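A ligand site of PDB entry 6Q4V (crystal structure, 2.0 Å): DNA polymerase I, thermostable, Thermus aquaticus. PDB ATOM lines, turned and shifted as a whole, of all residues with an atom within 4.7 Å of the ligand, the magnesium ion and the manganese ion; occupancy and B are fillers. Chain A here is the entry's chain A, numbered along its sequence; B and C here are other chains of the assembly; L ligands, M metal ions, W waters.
The magnesium ion is bound by the side-chain carboxylate (OD1) of Asp 494, the side-chain carboxylate (OD2) of Asp 319, water W5 and an oxygen (O7) of the ligand. The magnesium ion has four donor atoms within binding distance. Slightly farther from the magnesium ion lies water W6 (2.6 Å).
N2 of DG 5 of chain B sits close to N5 of the ligand, 3.4 Å away. Merely in contact with the ligand: Ser 321 and Phe 376. 15 residues have an atom within 4 Å of the ligand: Arg 282, Asp 319, Tyr 320, Ser 321, Gln 322, Ile 323, Glu 324, His 348, Arg 368, Lys 372, Phe 376, Asp 494, DT 4 of chain B, DG 5 of chain B and DOC 12 of chain C.
Three residues have an atom within 4 Å of the manganese ion: Asp 319, Tyr 320 and Asp 494. Along chain A the residues within 4 Å of the manganese ion span positions 319 to 494. The nearest printed residue that does not touch the manganese ion is Ser 321 (4.4 Å).
Water W5 lies within hydrogen-bond range of OE1 of Glu 495 (2.7 Å) and O of Val 492 (2.9 Å). Water W6 lies within hydrogen-bond range of an oxygen (O8) of the ligand (2.8 Å) and OP1 of DOC 12 of chain C (3.1 Å). Water W7 bridges OP2 of DOC 12 of chain C (2.8 Å) and O8 of the ligand (3.0 Å). Water W1 bridges an oxygen (O3) of the ligand (3.0 Å) and the side-chain amino group of Lys 372 (3.2 Å). Water W3 lies within hydrogen-bond range of OE1 of Glu 324 (2.8 Å) and N5 of the ligand (3.2 Å).
The side-chain carboxylate (OD2) of Asp 319 lies close to the side-chain amino group (NZ) of Lys 540, at 3.1 Å. O2 of DOC 12 of chain C lies within hydrogen-bond range of the guanidinium group (NH1) of Arg 282 (2.8 Å). N2 of DG 5 of chain B sits close to O2 of DOC 12 of chain C. The side-chain carboxylate of Glu 324 lies within salt-bridge range of the guanidinium group of Arg 282 (3.8 Å). The side-chain carboxylate (OE1) of Glu 324 lies within hydrogen-bond range of the side-chain hydroxyl (OH) of Tyr 380, at 2.5 Å.
The manganese ion is bound by OD2 of Asp 494, at 2.0 Å. The manganese ion is bound by O4 of the ligand (2.1 Å). The manganese ion is bound by OD1 of Asp 319 (2.2 Å). The manganese ion is bound by an oxygen (O1) of the ligand (2.2 Å). The manganese ion is bound by O of Tyr 320 (2.2 Å). An oxygen (O7) of the ligand binds the manganese ion (2.2 Å).
DOC 12 of chain C touches the magnesium ion (C3' to MG, 3.7 Å). Three residues have an atom within 4 Å of the magnesium ion: Asp 319, Asp 494 and DOC 12 of chain C.
O4 of DT 4 of chain B is in hydrogen-bond range of a nitrogen (N3) of the ligand, at 2.9 Å. The side-chain amino group (NZ) of Lys 372 lies within salt-bridge range of an oxygen (O3) of the ligand, at 2.8 Å. NH1 of Arg 368 is in salt-bridge range of O3 of the ligand. N of Gln 322 lies within hydrogen-bond range of O2 of the ligand (3.0 Å). An oxygen (O5) of the ligand sits at hydrogen-bond distance from a ring nitrogen (NE2) of His 348 (3.0 Å). N4 of DOC 12 of chain C sits at hydrogen-bond distance from N3 of the ligand, at 3.5 Å. The backbone NH of Ile 323 sits close to an oxygen (O4) of the ligand. N of Glu 324 sits at hydrogen-bond distance from O12 of the ligand, at 3.1 Å. The guanidinium group (NH2) of Arg 282 is in hydrogen-bond range of an oxygen (O11) of the ligand, 3.3 Å away.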
ATOM      1  N   ARG A 282       2.470 -10.406  -9.099  1.00  0.00           N
ATOM      2  CA  ARG A 282       2.239 -10.485 -10.531  1.00  0.00           C
ATOM      3  C   ARG A 282       0.854  -9.959 -10.870  1.00  0.00           C
ATOM      4  O   ARG A 282      -0.062  -9.917 -10.038  1.00  0.00           O
ATOM      5  CB  ARG A 282       2.356 -11.928 -11.014  1.00  0.00           C
ATOM      6  CG  ARG A 282       3.765 -12.436 -11.257  1.00  0.00           C
ATOM      7  CD  ARG A 282       3.696 -13.757 -12.012  1.00  0.00           C
ATOM      8  NE  ARG A 282       5.000 -14.220 -12.486  1.00  0.00           N
ATOM      9  CZ  ARG A 282       5.178 -15.367 -13.137  1.00  0.00           C
ATOM     10  NH1 ARG A 282       4.155 -16.173 -13.372  1.00  0.00           N
ATOM     11  NH2 ARG A 282       6.394 -15.707 -13.537  1.00  0.00           N
ATOM     12  N   ASP A 319      11.513  -8.758 -23.729  1.00  0.00           N
ATOM     13  CA  ASP A 319      11.467  -9.846 -22.755  1.00  0.00           C
ATOM     14  C   ASP A 319      12.774  -9.873 -21.987  1.00  0.00           C
ATOM     15  O   ASP A 319      13.841 -10.034 -22.594  1.00  0.00           O
ATOM     16  CB  ASP A 319      11.212 -11.180 -23.462  1.00  0.00           C
ATOM     17  CG  ASP A 319      11.026 -12.336 -22.491  1.00  0.00           C
ATOM     18  OD1 ASP A 319      11.889 -12.541 -21.614  1.00  0.00           O
ATOM     19  OD2 ASP A 319      10.004 -13.043 -22.611  1.00  0.00           O
ATOM     20  N   TYR A 320      12.694  -9.748 -20.659  1.00  0.00           N
ATOM     21  CA  TYR A 320      13.898  -9.799 -19.834  1.00  0.00           C
ATOM     22  C   TYR A 320      14.587 -11.146 -19.972  1.00  0.00           C
ATOM     23  O   TYR A 320      13.926 -12.186 -20.088  1.00  0.00           O
ATOM     24  CB  TYR A 320      13.550  -9.548 -18.366  1.00  0.00           C
ATOM     25  CG  TYR A 320      13.286  -8.105 -18.003  1.00  0.00           C
ATOM     26  CD1 TYR A 320      14.328  -7.192 -17.883  1.00  0.00           C
ATOM     27  CD2 TYR A 320      11.995  -7.653 -17.751  1.00  0.00           C
ATOM     28  CE1 TYR A 320      14.099  -5.868 -17.543  1.00  0.00           C
ATOM     29  CE2 TYR A 320      11.754  -6.336 -17.412  1.00  0.00           C
ATOM     30  CZ  TYR A 320      12.809  -5.456 -17.307  1.00  0.00           C
ATOM     31  OH  TYR A 320      12.568  -4.139 -16.968  1.00  0.00           O
ATOM     32  N   SER A 321      15.911 -11.137 -19.948  1.00  0.00           N
ATOM     33  CA  SER A 321      16.705 -12.359 -20.053  1.00  0.00           C
ATOM     34  C   SER A 321      16.889 -12.984 -18.668  1.00  0.00           C
ATOM     35  O   SER A 321      17.316 -12.305 -17.726  1.00  0.00           O
ATOM     36  CB  SER A 321      18.062 -12.064 -20.689  1.00  0.00           C
ATOM     37  OG  SER A 321      19.113 -12.651 -19.935  1.00  0.00           O
ATOM     38  N   GLN A 322      16.569 -14.269 -18.562  1.00  0.00           N
ATOM     39  CA  GLN A 322      16.824 -15.064 -17.361  1.00  0.00           C
ATOM     40  C   GLN A 322      16.454 -14.292 -16.094  1.00  0.00           C
ATOM     41  O   GLN A 322      17.236 -14.199 -15.144  1.00  0.00           O
ATOM     42  CB  GLN A 322      18.281 -15.504 -17.296  1.00  0.00           C
ATOM     43  CG  GLN A 322      18.858 -16.059 -18.585  1.00  0.00           C
ATOM     44  CD  GLN A 322      20.362 -16.258 -18.492  1.00  0.00           C
ATOM     45  OE1 GLN A 322      21.123 -15.702 -19.281  1.00  0.00           O
ATOM     46  NE2 GLN A 322      20.785 -17.055 -17.512  1.00  0.00           N
ATOM     47  N   ILE A 323      15.242 -13.740 -16.073  1.00  0.00           N
ATOM     48  CA  ILE A 323      14.968 -12.625 -15.173  1.00  0.00           C
ATOM     49  C   ILE A 323      15.086 -13.045 -13.711  1.00  0.00           C
ATOM     50  O   ILE A 323      15.822 -12.435 -12.934  1.00  0.00           O
ATOM     51  CB  ILE A 323      13.602 -11.985 -15.489  1.00  0.00           C
ATOM     52  CG1 ILE A 323      13.395 -10.750 -14.600  1.00  0.00           C
ATOM     53  CG2 ILE A 323      12.464 -12.975 -15.303  1.00  0.00           C
ATOM     54  CD1 ILE A 323      14.525  -9.741 -14.683  1.00  0.00           C
ATOM     55  N   GLU A 324      14.362 -14.102 -13.306  1.00  0.00           N
ATOM     56  CA  GLU A 324      14.357 -14.445 -11.889  1.00  0.00           C
ATOM     57  C   GLU A 324      15.697 -14.999 -11.425  1.00  0.00           C
ATOM     58  O   GLU A 324      15.969 -14.987 -10.225  1.00  0.00           O
ATOM     59  CB  GLU A 324      13.219 -15.426 -11.591  1.00  0.00           C
ATOM     60  CG  GLU A 324      11.881 -14.700 -11.360  1.00  0.00           C
ATOM     61  CD  GLU A 324      10.711 -15.628 -11.098  1.00  0.00           C
ATOM     62  OE1 GLU A 324      10.885 -16.652 -10.394  1.00  0.00           O
ATOM     63  OE2 GLU A 324       9.604 -15.336 -11.589  1.00  0.00           O
ATOM     64  N   HIS A 348      20.187 -21.194 -19.001  1.00  0.00           N
ATOM     65  CA  HIS A 348      19.203 -22.011 -19.704  1.00  0.00           C
ATOM     66  C   HIS A 348      19.842 -22.723 -20.886  1.00  0.00           C
ATOM     67  O   HIS A 348      19.580 -23.910 -21.121  1.00  0.00           O
ATOM     68  CB  HIS A 348      18.030 -21.139 -20.161  1.00  0.00           C
ATOM     69  CG  HIS A 348      17.321 -20.459 -19.034  1.00  0.00           C
ATOM     70  ND1 HIS A 348      17.248 -21.003 -17.763  1.00  0.00           N
ATOM     71  CD2 HIS A 348      16.648 -19.280 -18.972  1.00  0.00           C
ATOM     72  CE1 HIS A 348      16.559 -20.194 -16.982  1.00  0.00           C
ATOM     73  NE2 HIS A 348      16.192 -19.142 -17.683  1.00  0.00           N
ATOM     74  N   ARG A 368      15.941 -25.218 -25.165  1.00  0.00           N
ATOM     75  CA  ARG A 368      16.112 -24.233 -24.097  1.00  0.00           C
ATOM     76  C   ARG A 368      14.839 -24.102 -23.266  1.00  0.00           C
ATOM     77  O   ARG A 368      14.903 -23.895 -22.045  1.00  0.00           O
ATOM     78  CB  ARG A 368      16.508 -22.883 -24.707  1.00  0.00           C
ATOM     79  CG  ARG A 368      17.149 -21.921 -23.725  1.00  0.00           C
ATOM     80  CD  ARG A 368      17.756 -20.728 -24.456  1.00  0.00           C
ATOM     81  NE  ARG A 368      18.048 -19.622 -23.557  1.00  0.00           N
ATOM     82  CZ  ARG A 368      17.141 -18.754 -23.098  1.00  0.00           C
ATOM     83  NH1 ARG A 368      15.875 -18.864 -23.460  1.00  0.00           N
ATOM     84  NH2 ARG A 368      17.513 -17.782 -22.281  1.00  0.00           N
ATOM     85  N   LYS A 372      14.564 -24.518 -18.992  1.00  0.00           N
ATOM     86  CA  LYS A 372      14.024 -23.555 -18.037  1.00  0.00           C
ATOM     87  C   LYS A 372      13.235 -24.255 -16.944  1.00  0.00           C
ATOM     88  O   LYS A 372      13.412 -23.973 -15.756  1.00  0.00           O
ATOM     89  CB  LYS A 372      13.157 -22.519 -18.749  1.00  0.00           C
ATOM     90  CG  LYS A 372      13.940 -21.371 -19.341  1.00  0.00           C
ATOM     91  CD  LYS A 372      13.041 -20.187 -19.658  1.00  0.00           C
ATOM     92  CE  LYS A 372      12.878 -19.999 -21.150  1.00  0.00           C
ATOM     93  NZ  LYS A 372      12.174 -18.726 -21.456  1.00  0.00           N
ATOM     94  N   THR A 373      12.338 -25.158 -17.334  1.00  0.00           N
ATOM     95  CA  THR A 373      11.590 -25.918 -16.337  1.00  0.00           C
ATOM     96  C   THR A 373      12.533 -26.598 -15.355  1.00  0.00           C
ATOM     97  O   THR A 373      12.292 -26.610 -14.141  1.00  0.00           O
ATOM     98  CB  THR A 373      10.697 -26.947 -17.024  1.00  0.00           C
ATOM     99  OG1 THR A 373       9.965 -26.318 -18.085  1.00  0.00           O
ATOM    100  CG2 THR A 373       9.714 -27.560 -16.038  1.00  0.00           C
ATOM    101  N   PHE A 376      14.358 -23.818 -13.063  1.00  0.00           N
ATOM    102  CA  PHE A 376      13.455 -23.233 -12.083  1.00  0.00           C
ATOM    103  C   PHE A 376      12.797 -24.302 -11.209  1.00  0.00           C
ATOM    104  O   PHE A 376      12.491 -24.035 -10.048  1.00  0.00           O
ATOM    105  CB  PHE A 376      12.403 -22.370 -12.785  1.00  0.00           C
ATOM    106  CG  PHE A 376      12.978 -21.154 -13.456  1.00  0.00           C
ATOM    107  CD1 PHE A 376      13.610 -20.167 -12.710  1.00  0.00           C
ATOM    108  CD2 PHE A 376      12.914 -20.997 -14.831  1.00  0.00           C
ATOM    109  CE1 PHE A 376      14.155 -19.053 -13.319  1.00  0.00           C
ATOM    110  CE2 PHE A 376      13.461 -19.886 -15.449  1.00  0.00           C
ATOM    111  CZ  PHE A 376      14.079 -18.903 -14.694  1.00  0.00           C
ATOM    112  N   TYR A 380      13.349 -23.953  -7.118  1.00  0.00           N
ATOM    113  CA  TYR A 380      12.225 -23.796  -6.215  1.00  0.00           C
ATOM    114  C   TYR A 380      11.845 -25.096  -5.518  1.00  0.00           C
ATOM    115  O   TYR A 380      10.764 -25.178  -4.915  1.00  0.00           O
ATOM    116  CB  TYR A 380      11.035 -23.201  -6.974  1.00  0.00           C
ATOM    117  CG  TYR A 380      11.334 -21.784  -7.429  1.00  0.00           C
ATOM    118  CD1 TYR A 380      11.722 -20.817  -6.523  1.00  0.00           C
ATOM    119  CD2 TYR A 380      11.258 -21.424  -8.777  1.00  0.00           C
ATOM    120  CE1 TYR A 380      12.009 -19.531  -6.919  1.00  0.00           C
ATOM    121  CE2 TYR A 380      11.541 -20.131  -9.189  1.00  0.00           C
ATOM    122  CZ  TYR A 380      11.913 -19.192  -8.253  1.00  0.00           C
ATOM    123  OH  TYR A 380      12.206 -17.890  -8.631  1.00  0.00           O
ATOM    124  N   VAL A 492       3.217  -9.819 -20.283  1.00  0.00           N
ATOM    125  CA  VAL A 492       3.215 -11.246 -19.967  1.00  0.00           C
ATOM    126  C   VAL A 492       4.281 -11.503 -18.914  1.00  0.00           C
ATOM    127  O   VAL A 492       5.274 -12.185 -19.166  1.00  0.00           O
ATOM    128  CB  VAL A 492       3.438 -12.104 -21.229  1.00  0.00           C
ATOM    129  CG1 VAL A 492       3.246 -13.575 -20.921  1.00  0.00           C
ATOM    130  CG2 VAL A 492       2.488 -11.671 -22.339  1.00  0.00           C
ATOM    131  N   ASP A 494       7.117 -10.945 -17.576  1.00  0.00           N
ATOM    132  CA  ASP A 494       8.417 -10.330 -17.794  1.00  0.00           C
ATOM    133  C   ASP A 494       8.581  -9.842 -19.228  1.00  0.00           C
ATOM    134  O   ASP A 494       9.699  -9.628 -19.685  1.00  0.00           O
ATOM    135  CB  ASP A 494       9.542 -11.293 -17.414  1.00  0.00           C
ATOM    136  CG  ASP A 494       9.862 -12.285 -18.510  1.00  0.00           C
ATOM    137  OD1 ASP A 494       8.936 -12.677 -19.248  1.00  0.00           O
ATOM    138  OD2 ASP A 494      11.044 -12.652 -18.654  1.00  0.00           O
ATOM    139  N   GLU A 495       7.472  -9.666 -19.942  1.00  0.00           N
ATOM    140  CA  GLU A 495       7.487  -9.303 -21.354  1.00  0.00           C
ATOM    141  C   GLU A 495       6.459  -8.195 -21.597  1.00  0.00           C
ATOM    142  O   GLU A 495       5.416  -8.153 -20.960  1.00  0.00           O
ATOM    143  CB  GLU A 495       7.188 -10.532 -22.231  1.00  0.00           C
ATOM    144  CG  GLU A 495       6.938 -10.221 -23.707  1.00  0.00           C
ATOM    145  CD  GLU A 495       6.488 -11.454 -24.483  1.00  0.00           C
ATOM    146  OE1 GLU A 495       6.344 -12.528 -23.850  1.00  0.00           O
ATOM    147  OE2 GLU A 495       6.286 -11.351 -25.703  1.00  0.00           O
ATOM    148  N   LYS A 540       9.733 -12.045 -31.806  1.00  0.00           N
ATOM    149  CA  LYS A 540      10.615 -12.655 -30.808  1.00  0.00           C
ATOM    150  C   LYS A 540      11.609 -13.584 -31.475  1.00  0.00           C
ATOM    151  O   LYS A 540      12.550 -13.133 -32.130  1.00  0.00           O
ATOM    152  CB  LYS A 540       9.799 -13.416 -29.753  1.00  0.00           C
ATOM    153  CG  LYS A 540       9.028 -12.512 -28.790  1.00  0.00           C
ATOM    154  CD  LYS A 540       8.356 -13.279 -27.660  1.00  0.00           C
ATOM    155  CE  LYS A 540       9.353 -13.706 -26.583  1.00  0.00           C
ATOM    156  NZ  LYS A 540       8.701 -14.024 -25.281  1.00  0.00           N
ATOM    157  P    DT B   4       8.181 -31.944  -6.711  1.00  0.00           P
ATOM    158  OP1  DT B   4       7.074 -32.372  -7.609  1.00  0.00           O
ATOM    159  OP2  DT B   4       9.406 -32.759  -6.624  1.00  0.00           O
ATOM    160  O5'  DT B   4       8.636 -30.462  -7.099  1.00  0.00           O
ATOM    161  C5'  DT B   4       7.692 -29.406  -7.115  1.00  0.00           C
ATOM    162  C4'  DT B   4       8.362 -28.069  -6.884  1.00  0.00           C
ATOM    163  O4'  DT B   4       9.322 -27.825  -7.954  1.00  0.00           O
ATOM    164  C3'  DT B   4       7.431 -26.887  -6.910  1.00  0.00           C
ATOM    165  O3'  DT B   4       6.817 -26.670  -5.632  1.00  0.00           O
ATOM    166  C2'  DT B   4       8.347 -25.761  -7.330  1.00  0.00           C
ATOM    167  C1'  DT B   4       9.307 -26.448  -8.299  1.00  0.00           C
ATOM    168  N1   DT B   4       8.910 -26.302  -9.745  1.00  0.00           N
ATOM    169  C2   DT B   4       8.937 -25.058 -10.348  1.00  0.00           C
ATOM    170  O2   DT B   4       9.272 -24.043  -9.773  1.00  0.00           O
ATOM    171  N3   DT B   4       8.556 -25.051 -11.675  1.00  0.00           N
ATOM    172  C4   DT B   4       8.176 -26.131 -12.431  1.00  0.00           C
ATOM    173  O4   DT B   4       7.848 -26.030 -13.612  1.00  0.00           O
ATOM    174  C5   DT B   4       8.172 -27.404 -11.737  1.00  0.00           C
ATOM    175  C7   DT B   4       7.762 -28.651 -12.457  1.00  0.00           C
ATOM    176  C6   DT B   4       8.537 -27.423 -10.456  1.00  0.00           C
ATOM    177  P    DG B   5       5.241 -26.393  -5.520  1.00  0.00           P
ATOM    178  OP1  DG B   5       4.869 -26.552  -4.095  1.00  0.00           O
ATOM    179  OP2  DG B   5       4.557 -27.190  -6.573  1.00  0.00           O
ATOM    180  O5'  DG B   5       5.095 -24.836  -5.879  1.00  0.00           O
ATOM    181  C5'  DG B   5       5.646 -23.859  -4.992  1.00  0.00           C
ATOM    182  C4'  DG B   5       5.920 -22.549  -5.718  1.00  0.00           C
ATOM    183  O4'  DG B   5       6.765 -22.781  -6.876  1.00  0.00           O
ATOM    184  C3'  DG B   5       4.705 -21.858  -6.276  1.00  0.00           C
ATOM    185  O3'  DG B   5       4.020 -21.131  -5.268  1.00  0.00           O
ATOM    186  C2'  DG B   5       5.314 -20.967  -7.336  1.00  0.00           C
ATOM    187  C1'  DG B   5       6.451 -21.825  -7.873  1.00  0.00           C
ATOM    188  N9   DG B   5       6.090 -22.514  -9.113  1.00  0.00           N
ATOM    189  C8   DG B   5       5.853 -23.864  -9.284  1.00  0.00           C
ATOM    190  N7   DG B   5       5.546 -24.177 -10.513  1.00  0.00           N
ATOM    191  C5   DG B   5       5.578 -22.962 -11.193  1.00  0.00           C
ATOM    192  C6   DG B   5       5.322 -22.661 -12.551  1.00  0.00           C
ATOM    193  O6   DG B   5       5.020 -23.448 -13.468  1.00  0.00           O
ATOM    194  N1   DG B   5       5.465 -21.301 -12.811  1.00  0.00           N
ATOM    195  C2   DG B   5       5.800 -20.355 -11.889  1.00  0.00           C
ATOM    196  N2   DG B   5       5.885 -19.090 -12.332  1.00  0.00           N
ATOM    197  N3   DG B   5       6.040 -20.626 -10.610  1.00  0.00           N
ATOM    198  C4   DG B   5       5.907 -21.939 -10.334  1.00  0.00           C
ATOM    199  N1  DOC C  12       5.408 -18.557 -17.148  1.00  0.00           N
ATOM    200  C2  DOC C  12       5.430 -19.121 -15.824  1.00  0.00           C
ATOM    201  N3  DOC C  12       5.476 -20.591 -15.668  1.00  0.00           N
ATOM    202  C4  DOC C  12       5.510 -21.385 -16.712  1.00  0.00           C
ATOM    203  C5  DOC C  12       5.501 -20.785 -18.107  1.00  0.00           C
ATOM    204  C6  DOC C  12       5.453 -19.392 -18.262  1.00  0.00           C
ATOM    205  O2  DOC C  12       5.393 -18.298 -14.737  1.00  0.00           O
ATOM    206  N4  DOC C  12       5.543 -22.810 -16.536  1.00  0.00           N
ATOM    207  C1' DOC C  12       5.334 -17.120 -17.356  1.00  0.00           C
ATOM    208  C2' DOC C  12       6.688 -16.474 -17.269  1.00  0.00           C
ATOM    209  C3' DOC C  12       7.036 -16.183 -18.719  1.00  0.00           C
ATOM    210  C4' DOC C  12       5.664 -16.060 -19.346  1.00  0.00           C
ATOM    211  O4' DOC C  12       4.788 -16.858 -18.584  1.00  0.00           O
ATOM    212  C5' DOC C  12       5.540 -16.468 -20.735  1.00  0.00           C
ATOM    213  O5' DOC C  12       6.002 -17.809 -20.930  1.00  0.00           O
ATOM    214  P   DOC C  12       5.766 -18.437 -22.343  1.00  0.00           P
ATOM    215  OP1 DOC C  12       6.263 -17.408 -23.426  1.00  0.00           O
ATOM    216  OP2 DOC C  12       6.539 -19.717 -22.474  1.00  0.00           O
HETATM  217  P1  LIG L   1      14.506 -15.973 -21.117  1.00  0.00           P
HETATM  218  O1  LIG L   1      13.592 -14.789 -21.184  1.00  0.00           O
HETATM  219  O2  LIG L   1      15.988 -15.613 -21.185  1.00  0.00           O
HETATM  220  O3  LIG L   1      14.208 -17.007 -22.215  1.00  0.00           O
HETATM  221  P2  LIG L   1      13.487 -16.311 -18.431  1.00  0.00           P
HETATM  222  O4  LIG L   1      13.290 -14.840 -18.325  1.00  0.00           O
HETATM  223  O5  LIG L   1      14.159 -16.944 -17.225  1.00  0.00           O
HETATM  224  O6  LIG L   1      14.309 -16.723 -19.730  1.00  0.00           O
HETATM  225  P3  LIG L   1      10.681 -16.552 -19.110  1.00  0.00           P
HETATM  226  O7  LIG L   1      10.761 -15.218 -19.727  1.00  0.00           O
HETATM  227  O8  LIG L   1      10.042 -17.627 -19.979  1.00  0.00           O
HETATM  228  O9  LIG L   1      12.114 -17.078 -18.675  1.00  0.00           O
HETATM  229  O10 LIG L   1       9.886 -16.529 -17.730  1.00  0.00           O
HETATM  230  C1  LIG L   1       9.974 -15.418 -16.809  1.00  0.00           C
HETATM  231  C2  LIG L   1      10.192 -15.940 -15.416  1.00  0.00           C
HETATM  232  O11 LIG L   1       9.090 -16.784 -15.021  1.00  0.00           O
HETATM  233  C3  LIG L   1      11.430 -16.807 -15.218  1.00  0.00           C
HETATM  234  O12 LIG L   1      12.589 -16.005 -14.971  1.00  0.00           O
HETATM  235  C4  LIG L   1      11.056 -17.601 -13.975  1.00  0.00           C
HETATM  236  C5  LIG L   1       9.557 -17.779 -14.116  1.00  0.00           C
HETATM  237  N1  LIG L   1       9.173 -19.090 -14.634  1.00  0.00           N
HETATM  238  C6  LIG L   1       9.041 -19.477 -15.943  1.00  0.00           C
HETATM  239  N2  LIG L   1       8.832 -20.753 -16.105  1.00  0.00           N
HETATM  240  C7  LIG L   1       8.822 -21.253 -14.811  1.00  0.00           C
HETATM  241  C8  LIG L   1       8.680 -22.548 -14.292  1.00  0.00           C
HETATM  242  N3  LIG L   1       8.559 -23.642 -15.047  1.00  0.00           N
HETATM  243  N4  LIG L   1       8.713 -22.696 -12.945  1.00  0.00           N
HETATM  244  C9  LIG L   1       8.886 -21.618 -12.188  1.00  0.00           C
HETATM  245  N5  LIG L   1       9.053 -20.341 -12.562  1.00  0.00           N
HETATM  246  C10 LIG L   1       9.017 -20.231 -13.892  1.00  0.00           C
HETATM  247 MG    MG M   1       8.969 -13.968 -20.901  1.00  0.00          MG
HETATM  248 MN    MN M   2      12.340 -13.662 -19.818  1.00  0.00          MN
HETATM  249  O   HOH W   1      11.495 -16.010 -23.078  1.00  0.00           O
HETATM  250  O   HOH W   2       9.071 -22.023 -18.592  1.00  0.00           O
HETATM  251  O   HOH W   3       8.549 -18.183 -10.211  1.00  0.00           O
HETATM  252  O   HOH W   4      14.278 -12.954 -22.952  1.00  0.00           O
HETATM  253  O   HOH W   5       6.666 -13.496 -21.313  1.00  0.00           O
HETATM  254  O   HOH W   6       8.841 -16.298 -22.105  1.00  0.00           O
HETATM  255  O   HOH W   7       8.660 -20.194 -20.750  1.00  0.00           O
